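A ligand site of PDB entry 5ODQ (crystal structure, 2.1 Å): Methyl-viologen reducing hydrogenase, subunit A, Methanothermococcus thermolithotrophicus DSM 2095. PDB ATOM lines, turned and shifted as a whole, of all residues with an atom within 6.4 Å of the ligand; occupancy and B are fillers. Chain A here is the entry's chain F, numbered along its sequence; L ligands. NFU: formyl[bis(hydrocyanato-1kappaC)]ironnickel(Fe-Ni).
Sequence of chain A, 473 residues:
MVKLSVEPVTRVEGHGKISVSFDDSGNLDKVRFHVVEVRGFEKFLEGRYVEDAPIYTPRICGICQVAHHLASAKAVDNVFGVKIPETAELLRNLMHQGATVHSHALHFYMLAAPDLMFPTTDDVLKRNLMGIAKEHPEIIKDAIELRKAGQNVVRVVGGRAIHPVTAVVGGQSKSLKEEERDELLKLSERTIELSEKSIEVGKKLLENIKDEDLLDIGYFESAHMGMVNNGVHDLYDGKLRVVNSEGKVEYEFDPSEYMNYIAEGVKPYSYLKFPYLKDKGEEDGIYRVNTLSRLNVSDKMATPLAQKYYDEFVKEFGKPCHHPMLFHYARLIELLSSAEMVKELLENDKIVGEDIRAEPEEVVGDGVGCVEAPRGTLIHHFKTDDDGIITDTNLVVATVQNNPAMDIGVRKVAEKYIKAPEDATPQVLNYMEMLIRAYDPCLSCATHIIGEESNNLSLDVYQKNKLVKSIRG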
ATOM      1  N   GLU A  13       9.918   1.717  -8.492  1.00  0.00           N
ATOM      2  CA  GLU A  13       9.069   2.031  -7.361  1.00  0.00           C
ATOM      3  C   GLU A  13       9.894   2.924  -6.461  1.00  0.00           C
ATOM      4  O   GLU A  13      11.037   2.615  -6.177  1.00  0.00           O
ATOM      5  CB  GLU A  13       8.653   0.757  -6.591  1.00  0.00           C
ATOM      6  CG  GLU A  13       7.669   1.011  -5.447  1.00  0.00           C
ATOM      7  CD  GLU A  13       8.150   1.917  -4.331  1.00  0.00           C
ATOM      8  OE1 GLU A  13       9.310   1.779  -3.887  1.00  0.00           O
ATOM      9  OE2 GLU A  13       7.354   2.776  -3.903  1.00  0.00           O
ATOM     10  N   ILE A  60       5.449  -0.870   4.114  1.00  0.00           N
ATOM     11  CA  ILE A  60       6.767  -0.384   3.731  1.00  0.00           C
ATOM     12  C   ILE A  60       6.718  -0.309   2.214  1.00  0.00           C
ATOM     13  O   ILE A  60       7.342   0.563   1.617  1.00  0.00           O
ATOM     14  CB  ILE A  60       7.902  -1.318   4.220  1.00  0.00           C
ATOM     15  CG1 ILE A  60       8.062  -1.202   5.743  1.00  0.00           C
ATOM     16  CG2 ILE A  60       9.229  -0.983   3.528  1.00  0.00           C
ATOM     17  CD1 ILE A  60       8.942  -2.268   6.365  1.00  0.00           C
ATOM     18  N   CYS A  61       5.956  -1.212   1.577  1.00  0.00           N
ATOM     19  CA  CYS A  61       5.832  -1.216   0.119  1.00  0.00           C
ATOM     20  C   CYS A  61       4.567  -1.932  -0.338  1.00  0.00           C
ATOM     21  O   CYS A  61       4.230  -2.995   0.162  1.00  0.00           O
ATOM     22  CB  CYS A  61       7.068  -1.834  -0.516  1.00  0.00           C
ATOM     23  SG  CYS A  61       6.880  -2.166  -2.281  1.00  0.00           S
ATOM     24  N   GLY A  62       3.892  -1.325  -1.319  1.00  0.00           N
ATOM     25  CA  GLY A  62       2.652  -1.836  -1.893  1.00  0.00           C
ATOM     26  C   GLY A  62       2.840  -2.921  -2.935  1.00  0.00           C
ATOM     27  O   GLY A  62       1.847  -3.509  -3.375  1.00  0.00           O
ATOM     28  N   ILE A  63       4.088  -3.182  -3.359  1.00  0.00           N
ATOM     29  CA  ILE A  63       4.373  -4.226  -4.349  1.00  0.00           C
ATOM     30  C   ILE A  63       4.746  -5.518  -3.630  1.00  0.00           C
ATOM     31  O   ILE A  63       4.192  -6.568  -3.933  1.00  0.00           O
ATOM     32  CB  ILE A  63       5.523  -3.807  -5.304  1.00  0.00           C
ATOM     33  CG1 ILE A  63       5.132  -2.537  -6.078  1.00  0.00           C
ATOM     34  CG2 ILE A  63       5.861  -4.943  -6.267  1.00  0.00           C
ATOM     35  CD1 ILE A  63       6.233  -1.938  -6.909  1.00  0.00           C
ATOM     36  N   CYS A  64       5.689  -5.431  -2.682  1.00  0.00           N
ATOM     37  CA  CYS A  64       6.177  -6.578  -1.923  1.00  0.00           C
ATOM     38  C   CYS A  64       5.625  -6.627  -0.497  1.00  0.00           C
ATOM     39  O   CYS A  64       6.327  -7.076   0.401  1.00  0.00           O
ATOM     40  CB  CYS A  64       7.696  -6.559  -1.917  1.00  0.00           C
ATOM     41  SG  CYS A  64       8.400  -5.012  -1.285  1.00  0.00           S
ATOM     42  N   GLN A  65       4.393  -6.184  -0.285  1.00  0.00           N
ATOM     43  CA  GLN A  65       3.818  -6.206   1.062  1.00  0.00           C
ATOM     44  C   GLN A  65       3.754  -7.618   1.623  1.00  0.00           C
ATOM     45  O   GLN A  65       3.898  -7.808   2.829  1.00  0.00           O
ATOM     46  CB  GLN A  65       2.413  -5.565   1.121  1.00  0.00           C
ATOM     47  CG  GLN A  65       1.895  -4.978  -0.193  1.00  0.00           C
ATOM     48  CD  GLN A  65       1.212  -6.004  -1.052  1.00  0.00           C
ATOM     49  OE1 GLN A  65       0.792  -7.072  -0.592  1.00  0.00           O
ATOM     50  NE2 GLN A  65       1.034  -5.685  -2.324  1.00  0.00           N
ATOM     51  N   ALA A  67       5.895 -10.074   1.203  1.00  0.00           N
ATOM     52  CA  ALA A  67       7.220 -10.424   1.717  1.00  0.00           C
ATOM     53  C   ALA A  67       7.422  -9.892   3.136  1.00  0.00           C
ATOM     54  O   ALA A  67       7.941 -10.608   3.994  1.00  0.00           O
ATOM     55  CB  ALA A  67       8.295  -9.862   0.789  1.00  0.00           C
ATOM     56  N   HIS A  68       7.010  -8.637   3.377  1.00  0.00           N
ATOM     57  CA  HIS A  68       7.142  -8.023   4.693  1.00  0.00           C
ATOM     58  C   HIS A  68       6.208  -8.677   5.700  1.00  0.00           C
ATOM     59  O   HIS A  68       6.611  -8.936   6.826  1.00  0.00           O
ATOM     60  CB  HIS A  68       6.856  -6.521   4.590  1.00  0.00           C
ATOM     61  CG  HIS A  68       7.933  -5.762   3.879  1.00  0.00           C
ATOM     62  ND1 HIS A  68       9.154  -5.541   4.483  1.00  0.00           N
ATOM     63  CD2 HIS A  68       7.940  -5.222   2.649  1.00  0.00           C
ATOM     64  CE1 HIS A  68       9.874  -4.863   3.600  1.00  0.00           C
ATOM     65  NE2 HIS A  68       9.173  -4.654   2.478  1.00  0.00           N
ATOM     66  N   SER A 103       4.762  -9.620  -8.724  1.00  0.00           N
ATOM     67  CA  SER A 103       5.838  -8.640  -8.675  1.00  0.00           C
ATOM     68  C   SER A 103       6.782  -8.773  -9.886  1.00  0.00           C
ATOM     69  O   SER A 103       7.150  -7.763 -10.469  1.00  0.00           O
ATOM     70  CB  SER A 103       6.633  -8.802  -7.390  1.00  0.00           C
ATOM     71  OG  SER A 103       7.555  -7.737  -7.207  1.00  0.00           O
ATOM     72  N   ALA A 373      12.547 -11.690  -0.761  1.00  0.00           N
ATOM     73  CA  ALA A 373      11.501 -10.900  -1.376  1.00  0.00           C
ATOM     74  C   ALA A 373      11.792 -10.906  -2.861  1.00  0.00           C
ATOM     75  O   ALA A 373      12.923 -11.226  -3.247  1.00  0.00           O
ATOM     76  CB  ALA A 373      11.537  -9.481  -0.854  1.00  0.00           C
ATOM     77  N   PRO A 374      10.852 -10.545  -3.748  1.00  0.00           N
ATOM     78  CA  PRO A 374      11.186 -10.551  -5.181  1.00  0.00           C
ATOM     79  C   PRO A 374      12.411  -9.694  -5.534  1.00  0.00           C
ATOM     80  O   PRO A 374      12.991  -9.911  -6.590  1.00  0.00           O
ATOM     81  CB  PRO A 374       9.909 -10.038  -5.847  1.00  0.00           C
ATOM     82  CG  PRO A 374       8.827 -10.293  -4.854  1.00  0.00           C
ATOM     83  CD  PRO A 374       9.454 -10.128  -3.512  1.00  0.00           C
ATOM     84  N   ARG A 375      12.816  -8.750  -4.674  1.00  0.00           N
ATOM     85  CA  ARG A 375      13.959  -7.881  -4.954  1.00  0.00           C
ATOM     86  C   ARG A 375      15.200  -8.198  -4.142  1.00  0.00           C
ATOM     87  O   ARG A 375      16.194  -7.470  -4.234  1.00  0.00           O
ATOM     88  CB  ARG A 375      13.557  -6.426  -4.824  1.00  0.00           C
ATOM     89  CG  ARG A 375      12.647  -6.043  -5.963  1.00  0.00           C
ATOM     90  CD  ARG A 375      11.827  -4.799  -5.746  1.00  0.00           C
ATOM     91  NE  ARG A 375      10.938  -4.591  -6.891  1.00  0.00           N
ATOM     92  CZ  ARG A 375       9.752  -5.185  -7.037  1.00  0.00           C
ATOM     93  NH1 ARG A 375       9.292  -6.007  -6.105  1.00  0.00           N
ATOM     94  NH2 ARG A 375       9.017  -4.952  -8.116  1.00  0.00           N
ATOM     95  N   GLY A 376      15.167  -9.284  -3.364  1.00  0.00           N
ATOM     96  CA  GLY A 376      16.325  -9.672  -2.578  1.00  0.00           C
ATOM     97  C   GLY A 376      16.027 -10.133  -1.175  1.00  0.00           C
ATOM     98  O   GLY A 376      14.878 -10.106  -0.726  1.00  0.00           O
ATOM     99  N   THR A 377      17.084 -10.547  -0.483  1.00  0.00           N
ATOM    100  CA  THR A 377      17.001 -11.027   0.890  1.00  0.00           C
ATOM    101  C   THR A 377      16.317 -10.003   1.757  1.00  0.00           C
ATOM    102  O   THR A 377      16.680  -8.835   1.741  1.00  0.00           O
ATOM    103  CB  THR A 377      18.397 -11.322   1.408  1.00  0.00           C
ATOM    104  OG1 THR A 377      19.100 -12.118   0.441  1.00  0.00           O
ATOM    105  CG2 THR A 377      18.380 -12.040   2.747  1.00  0.00           C
ATOM    106  N   LEU A 378      15.311 -10.444   2.509  1.00  0.00           N
ATOM    107  CA  LEU A 378      14.568  -9.568   3.380  1.00  0.00           C
ATOM    108  C   LEU A 378      14.720 -10.059   4.789  1.00  0.00           C
ATOM    109  O   LEU A 378      14.387 -11.211   5.067  1.00  0.00           O
ATOM    110  CB  LEU A 378      13.094  -9.564   2.982  1.00  0.00           C
ATOM    111  CG  LEU A 378      12.165  -8.781   3.876  1.00  0.00           C
ATOM    112  CD1 LEU A 378      12.610  -7.340   3.999  1.00  0.00           C
ATOM    113  CD2 LEU A 378      10.748  -8.863   3.362  1.00  0.00           C
ATOM    114  N   ILE A 379      15.244  -9.215   5.671  1.00  0.00           N
ATOM    115  CA  ILE A 379      15.437  -9.580   7.062  1.00  0.00           C
ATOM    116  C   ILE A 379      14.752  -8.568   7.960  1.00  0.00           C
ATOM    117  O   ILE A 379      15.032  -7.380   7.862  1.00  0.00           O
ATOM    118  CB  ILE A 379      16.949  -9.686   7.391  1.00  0.00           C
ATOM    119  CG1 ILE A 379      17.574 -10.913   6.686  1.00  0.00           C
ATOM    120  CG2 ILE A 379      17.162  -9.793   8.918  1.00  0.00           C
ATOM    121  CD1 ILE A 379      18.968 -10.728   6.335  1.00  0.00           C
ATOM    122  N   HIS A 380      13.863  -9.048   8.845  1.00  0.00           N
ATOM    123  CA  HIS A 380      13.159  -8.230   9.810  1.00  0.00           C
ATOM    124  C   HIS A 380      13.677  -8.730  11.151  1.00  0.00           C
ATOM    125  O   HIS A 380      13.579  -9.923  11.415  1.00  0.00           O
ATOM    126  CB  HIS A 380      11.635  -8.453   9.761  1.00  0.00           C
ATOM    127  CG  HIS A 380      10.926  -7.799   8.605  1.00  0.00           C
ATOM    128  ND1 HIS A 380       9.548  -7.727   8.575  1.00  0.00           N
ATOM    129  CD2 HIS A 380      11.413  -7.210   7.496  1.00  0.00           C
ATOM    130  CE1 HIS A 380       9.241  -7.093   7.453  1.00  0.00           C
ATOM    131  NE2 HIS A 380      10.332  -6.772   6.767  1.00  0.00           N
ATOM    132  N   VAL A 396      16.795  -5.088   6.997  1.00  0.00           N
ATOM    133  CA  VAL A 396      17.735  -5.094   5.902  1.00  0.00           C
ATOM    134  C   VAL A 396      16.809  -5.486   4.768  1.00  0.00           C
ATOM    135  O   VAL A 396      16.476  -6.658   4.616  1.00  0.00           O
ATOM    136  CB  VAL A 396      18.892  -6.088   6.111  1.00  0.00           C
ATOM    137  CG1 VAL A 396      20.010  -5.838   5.106  1.00  0.00           C
ATOM    138  CG2 VAL A 396      19.431  -5.986   7.549  1.00  0.00           C
ATOM    139  N   VAL A 397      16.334  -4.477   4.019  1.00  0.00           N
ATOM    140  CA  VAL A 397      15.358  -4.696   2.957  1.00  0.00           C
ATOM    141  C   VAL A 397      15.911  -4.749   1.557  1.00  0.00           C
ATOM    142  O   VAL A 397      16.359  -3.745   1.004  1.00  0.00           O
ATOM    143  CB  VAL A 397      14.255  -3.635   3.055  1.00  0.00           C
ATOM    144  CG1 VAL A 397      13.099  -3.977   2.112  1.00  0.00           C
ATOM    145  CG2 VAL A 397      13.741  -3.502   4.491  1.00  0.00           C
ATOM    146  N   ALA A 398      15.827  -5.944   0.971  1.00  0.00           N
ATOM    147  CA  ALA A 398      16.219  -6.312  -0.378  1.00  0.00           C
ATOM    148  C   ALA A 398      17.025  -5.302  -1.207  1.00  0.00           C
ATOM    149  O   ALA A 398      18.251  -5.409  -1.264  1.00  0.00           O
ATOM    150  CB  ALA A 398      14.987  -6.717  -1.141  1.00  0.00           C
ATOM    151  N   THR A 399      16.354  -4.350  -1.877  1.00  0.00           N
ATOM    152  CA  THR A 399      17.026  -3.386  -2.755  1.00  0.00           C
ATOM    153  C   THR A 399      18.196  -2.624  -2.149  1.00  0.00           C
ATOM    154  O   THR A 399      19.141  -2.344  -2.877  1.00  0.00           O
ATOM    155  CB  THR A 399      16.016  -2.425  -3.371  1.00  0.00           C
ATOM    156  OG1 THR A 399      15.244  -3.163  -4.327  1.00  0.00           O
ATOM    157  CG2 THR A 399      16.684  -1.259  -4.086  1.00  0.00           C
ATOM    158  N   VAL A 400      18.178  -2.292  -0.864  1.00  0.00           N
ATOM    159  CA  VAL A 400      19.298  -1.550  -0.278  1.00  0.00           C
ATOM    160  C   VAL A 400      20.637  -2.231  -0.639  1.00  0.00           C
ATOM    161  O   VAL A 400      21.635  -1.553  -0.840  1.00  0.00           O
ATOM    162  CB  VAL A 400      19.144  -1.368   1.260  1.00  0.00           C
ATOM    163  CG1 VAL A 400      19.278  -2.694   2.007  1.00  0.00           C
ATOM    164  CG2 VAL A 400      20.167  -0.358   1.788  1.00  0.00           C
ATOM    165  N   ASP A 440      15.409  -3.934 -10.708  1.00  0.00           N
ATOM    166  CA  ASP A 440      14.030  -3.892 -10.222  1.00  0.00           C
ATOM    167  C   ASP A 440      14.003  -3.241  -8.842  1.00  0.00           C
ATOM    168  O   ASP A 440      13.595  -3.859  -7.868  1.00  0.00           O
ATOM    169  CB  ASP A 440      13.417  -5.309 -10.180  1.00  0.00           C
ATOM    170  CG  ASP A 440      11.958  -5.358  -9.770  1.00  0.00           C
ATOM    171  OD1 ASP A 440      11.308  -4.291  -9.741  1.00  0.00           O
ATOM    172  OD2 ASP A 440      11.462  -6.458  -9.470  1.00  0.00           O
ATOM    173  N   PRO A 441      14.443  -1.985  -8.731  1.00  0.00           N
ATOM    174  CA  PRO A 441      14.460  -1.329  -7.423  1.00  0.00           C
ATOM    175  C   PRO A 441      13.116  -0.875  -6.888  1.00  0.00           C
ATOM    176  O   PRO A 441      12.228  -0.470  -7.632  1.00  0.00           O
ATOM    177  CB  PRO A 441      15.410  -0.155  -7.630  1.00  0.00           C
ATOM    178  CG  PRO A 441      15.289   0.179  -9.054  1.00  0.00           C
ATOM    179  CD  PRO A 441      14.984  -1.105  -9.780  1.00  0.00           C
ATOM    180  N   CYS A 442      12.987  -0.956  -5.577  1.00  0.00           N
ATOM    181  CA  CYS A 442      11.808  -0.558  -4.815  1.00  0.00           C
ATOM    182  C   CYS A 442      12.436   0.327  -3.736  1.00  0.00           C
ATOM    183  O   CYS A 442      12.848  -0.143  -2.679  1.00  0.00           O
ATOM    184  CB  CYS A 442      11.114  -1.782  -4.237  1.00  0.00           C
ATOM    185  SG  CYS A 442       9.493  -1.444  -3.504  1.00  0.00           S
ATOM    186  N   LEU A 443      12.541   1.619  -4.065  1.00  0.00           N
ATOM    187  CA  LEU A 443      13.172   2.625  -3.217  1.00  0.00           C
ATOM    188  C   LEU A 443      12.415   2.955  -1.931  1.00  0.00           C
ATOM    189  O   LEU A 443      13.047   3.403  -0.962  1.00  0.00           O
ATOM    190  CB  LEU A 443      13.484   3.884  -4.052  1.00  0.00           C
ATOM    191  CG  LEU A 443      14.224   3.588  -5.385  1.00  0.00           C
ATOM    192  CD1 LEU A 443      14.280   4.803  -6.277  1.00  0.00           C
ATOM    193  CD2 LEU A 443      15.630   3.072  -5.131  1.00  0.00           C
ATOM    194  N   SER A 444      11.104   2.715  -1.867  1.00  0.00           N
ATOM    195  CA  SER A 444      10.358   2.965  -0.636  1.00  0.00           C
ATOM    196  C   SER A 444      10.729   1.826   0.322  1.00  0.00           C
ATOM    197  O   SER A 444      10.917   2.036   1.518  1.00  0.00           O
ATOM    198  CB  SER A 444       8.854   2.954  -0.906  1.00  0.00           C
ATOM    199  OG  SER A 444       8.492   4.017  -1.776  1.00  0.00           O
ATOM    200  N   CYS A 445      10.879   0.633  -0.240  1.00  0.00           N
ATOM    201  CA  CYS A 445      11.251  -0.601   0.456  1.00  0.00           C
ATOM    202  C   CYS A 445      12.672  -0.523   0.991  1.00  0.00           C
ATOM    203  O   CYS A 445      12.913  -0.810   2.163  1.00  0.00           O
ATOM    204  CB  CYS A 445      11.109  -1.782  -0.494  1.00  0.00           C
ATOM    205  SG  CYS A 445      10.192  -3.174   0.194  1.00  0.00           S
ATOM    206  N   ALA A 446      13.603  -0.130   0.131  1.00  0.00           N
ATOM    207  CA  ALA A 446      15.030  -0.019   0.440  1.00  0.00           C
ATOM    208  C   ALA A 446      15.360   0.943   1.579  1.00  0.00           C
ATOM    209  O   ALA A 446      16.325   0.713   2.301  1.00  0.00           O
ATOM    210  CB  ALA A 446      15.770   0.406  -0.807  1.00  0.00           C
HETATM  211 FE   NFU L   1      10.651  -5.055  -1.237  1.00  0.00          FE
HETATM  212 NI   NFU L   1       8.981  -3.314  -2.315  1.00  0.00          NI
HETATM  213  C1  NFU L   1      10.585  -6.223  -2.633  1.00  0.00           C
HETATM  214  N1  NFU L   1      10.542  -6.981  -3.499  1.00  0.00           N
HETATM  215  C2  NFU L   1      12.131  -4.335  -1.996  1.00  0.00           C
HETATM  216  N2  NFU L   1      13.088  -3.879  -2.442  1.00  0.00           N
HETATM  217  C3  NFU L   1      11.289  -6.085   0.117  1.00  0.00           C
HETATM  218  O3  NFU L   1      11.722  -6.774   1.005  1.00  0.00           O
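Merely in contact with the ligand: Leu 378 (3.2 Å), Ala 373 (3.3 Å), Val 397 (3.3 Å), Pro 374 (3.3 Å), His 68 (3.5 Å) and Ala 398 (3.7 Å).
NE2 of His 68 sits close to SG of Cys 445 (2.9 Å).
The side-chain carboxylate of Glu 13 sits close to the side-chain sulfur of Cys 442.
NH1 of Arg 375 sits at hydrogen-bond distance from OG of Ser 103 (2.7 Å).
N of Ala 398 sits at hydrogen-bond distance from O of Thr 377 (3.1 Å).
The side-chain carboxylate of Asp 440 lies within salt-bridge range of the guanidinium group of Arg 375 (2.9 Å).
SG of Cys 61 lies close to N of Ile 63.
ND1 of His 68 is in hydrogen-bond range of NE2 of His 380 (2.8 Å).
The backbone NH of Cys 442 sits at hydrogen-bond distance from the side-chain hydroxyl of Thr 399 (3.4 Å).
A nickel atom (NI) of the ligand is bound by the side-chain sulfur (SG) of Cys 61.
A nickel atom (NI) of the ligand is bound by the side-chain sulfur (SG) of Cys 64, at 2.1 Å.
The side-chain sulfur of Cys 445 is bound to an iron atom (FE) of the ligand (2.4 Å).
NI of the ligand is bound by SG of Cys 442, 2.3 Å away.
N2 of the ligand is in hydrogen-bond range of N of Thr 399 (3.3 Å).
A nitrogen (N1) of the ligand is in hydrogen-bond range of the guanidinium group (NH1) of Arg 375 (3.0 Å).
The backbone NH (N) of Arg 375 lies within hydrogen-bond range of a nitrogen (N1) of the ligand (3.1 Å).
The side-chain hydroxyl (OG1) of Thr 399 is in hydrogen-bond range of a nitrogen (N2) of the ligand.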
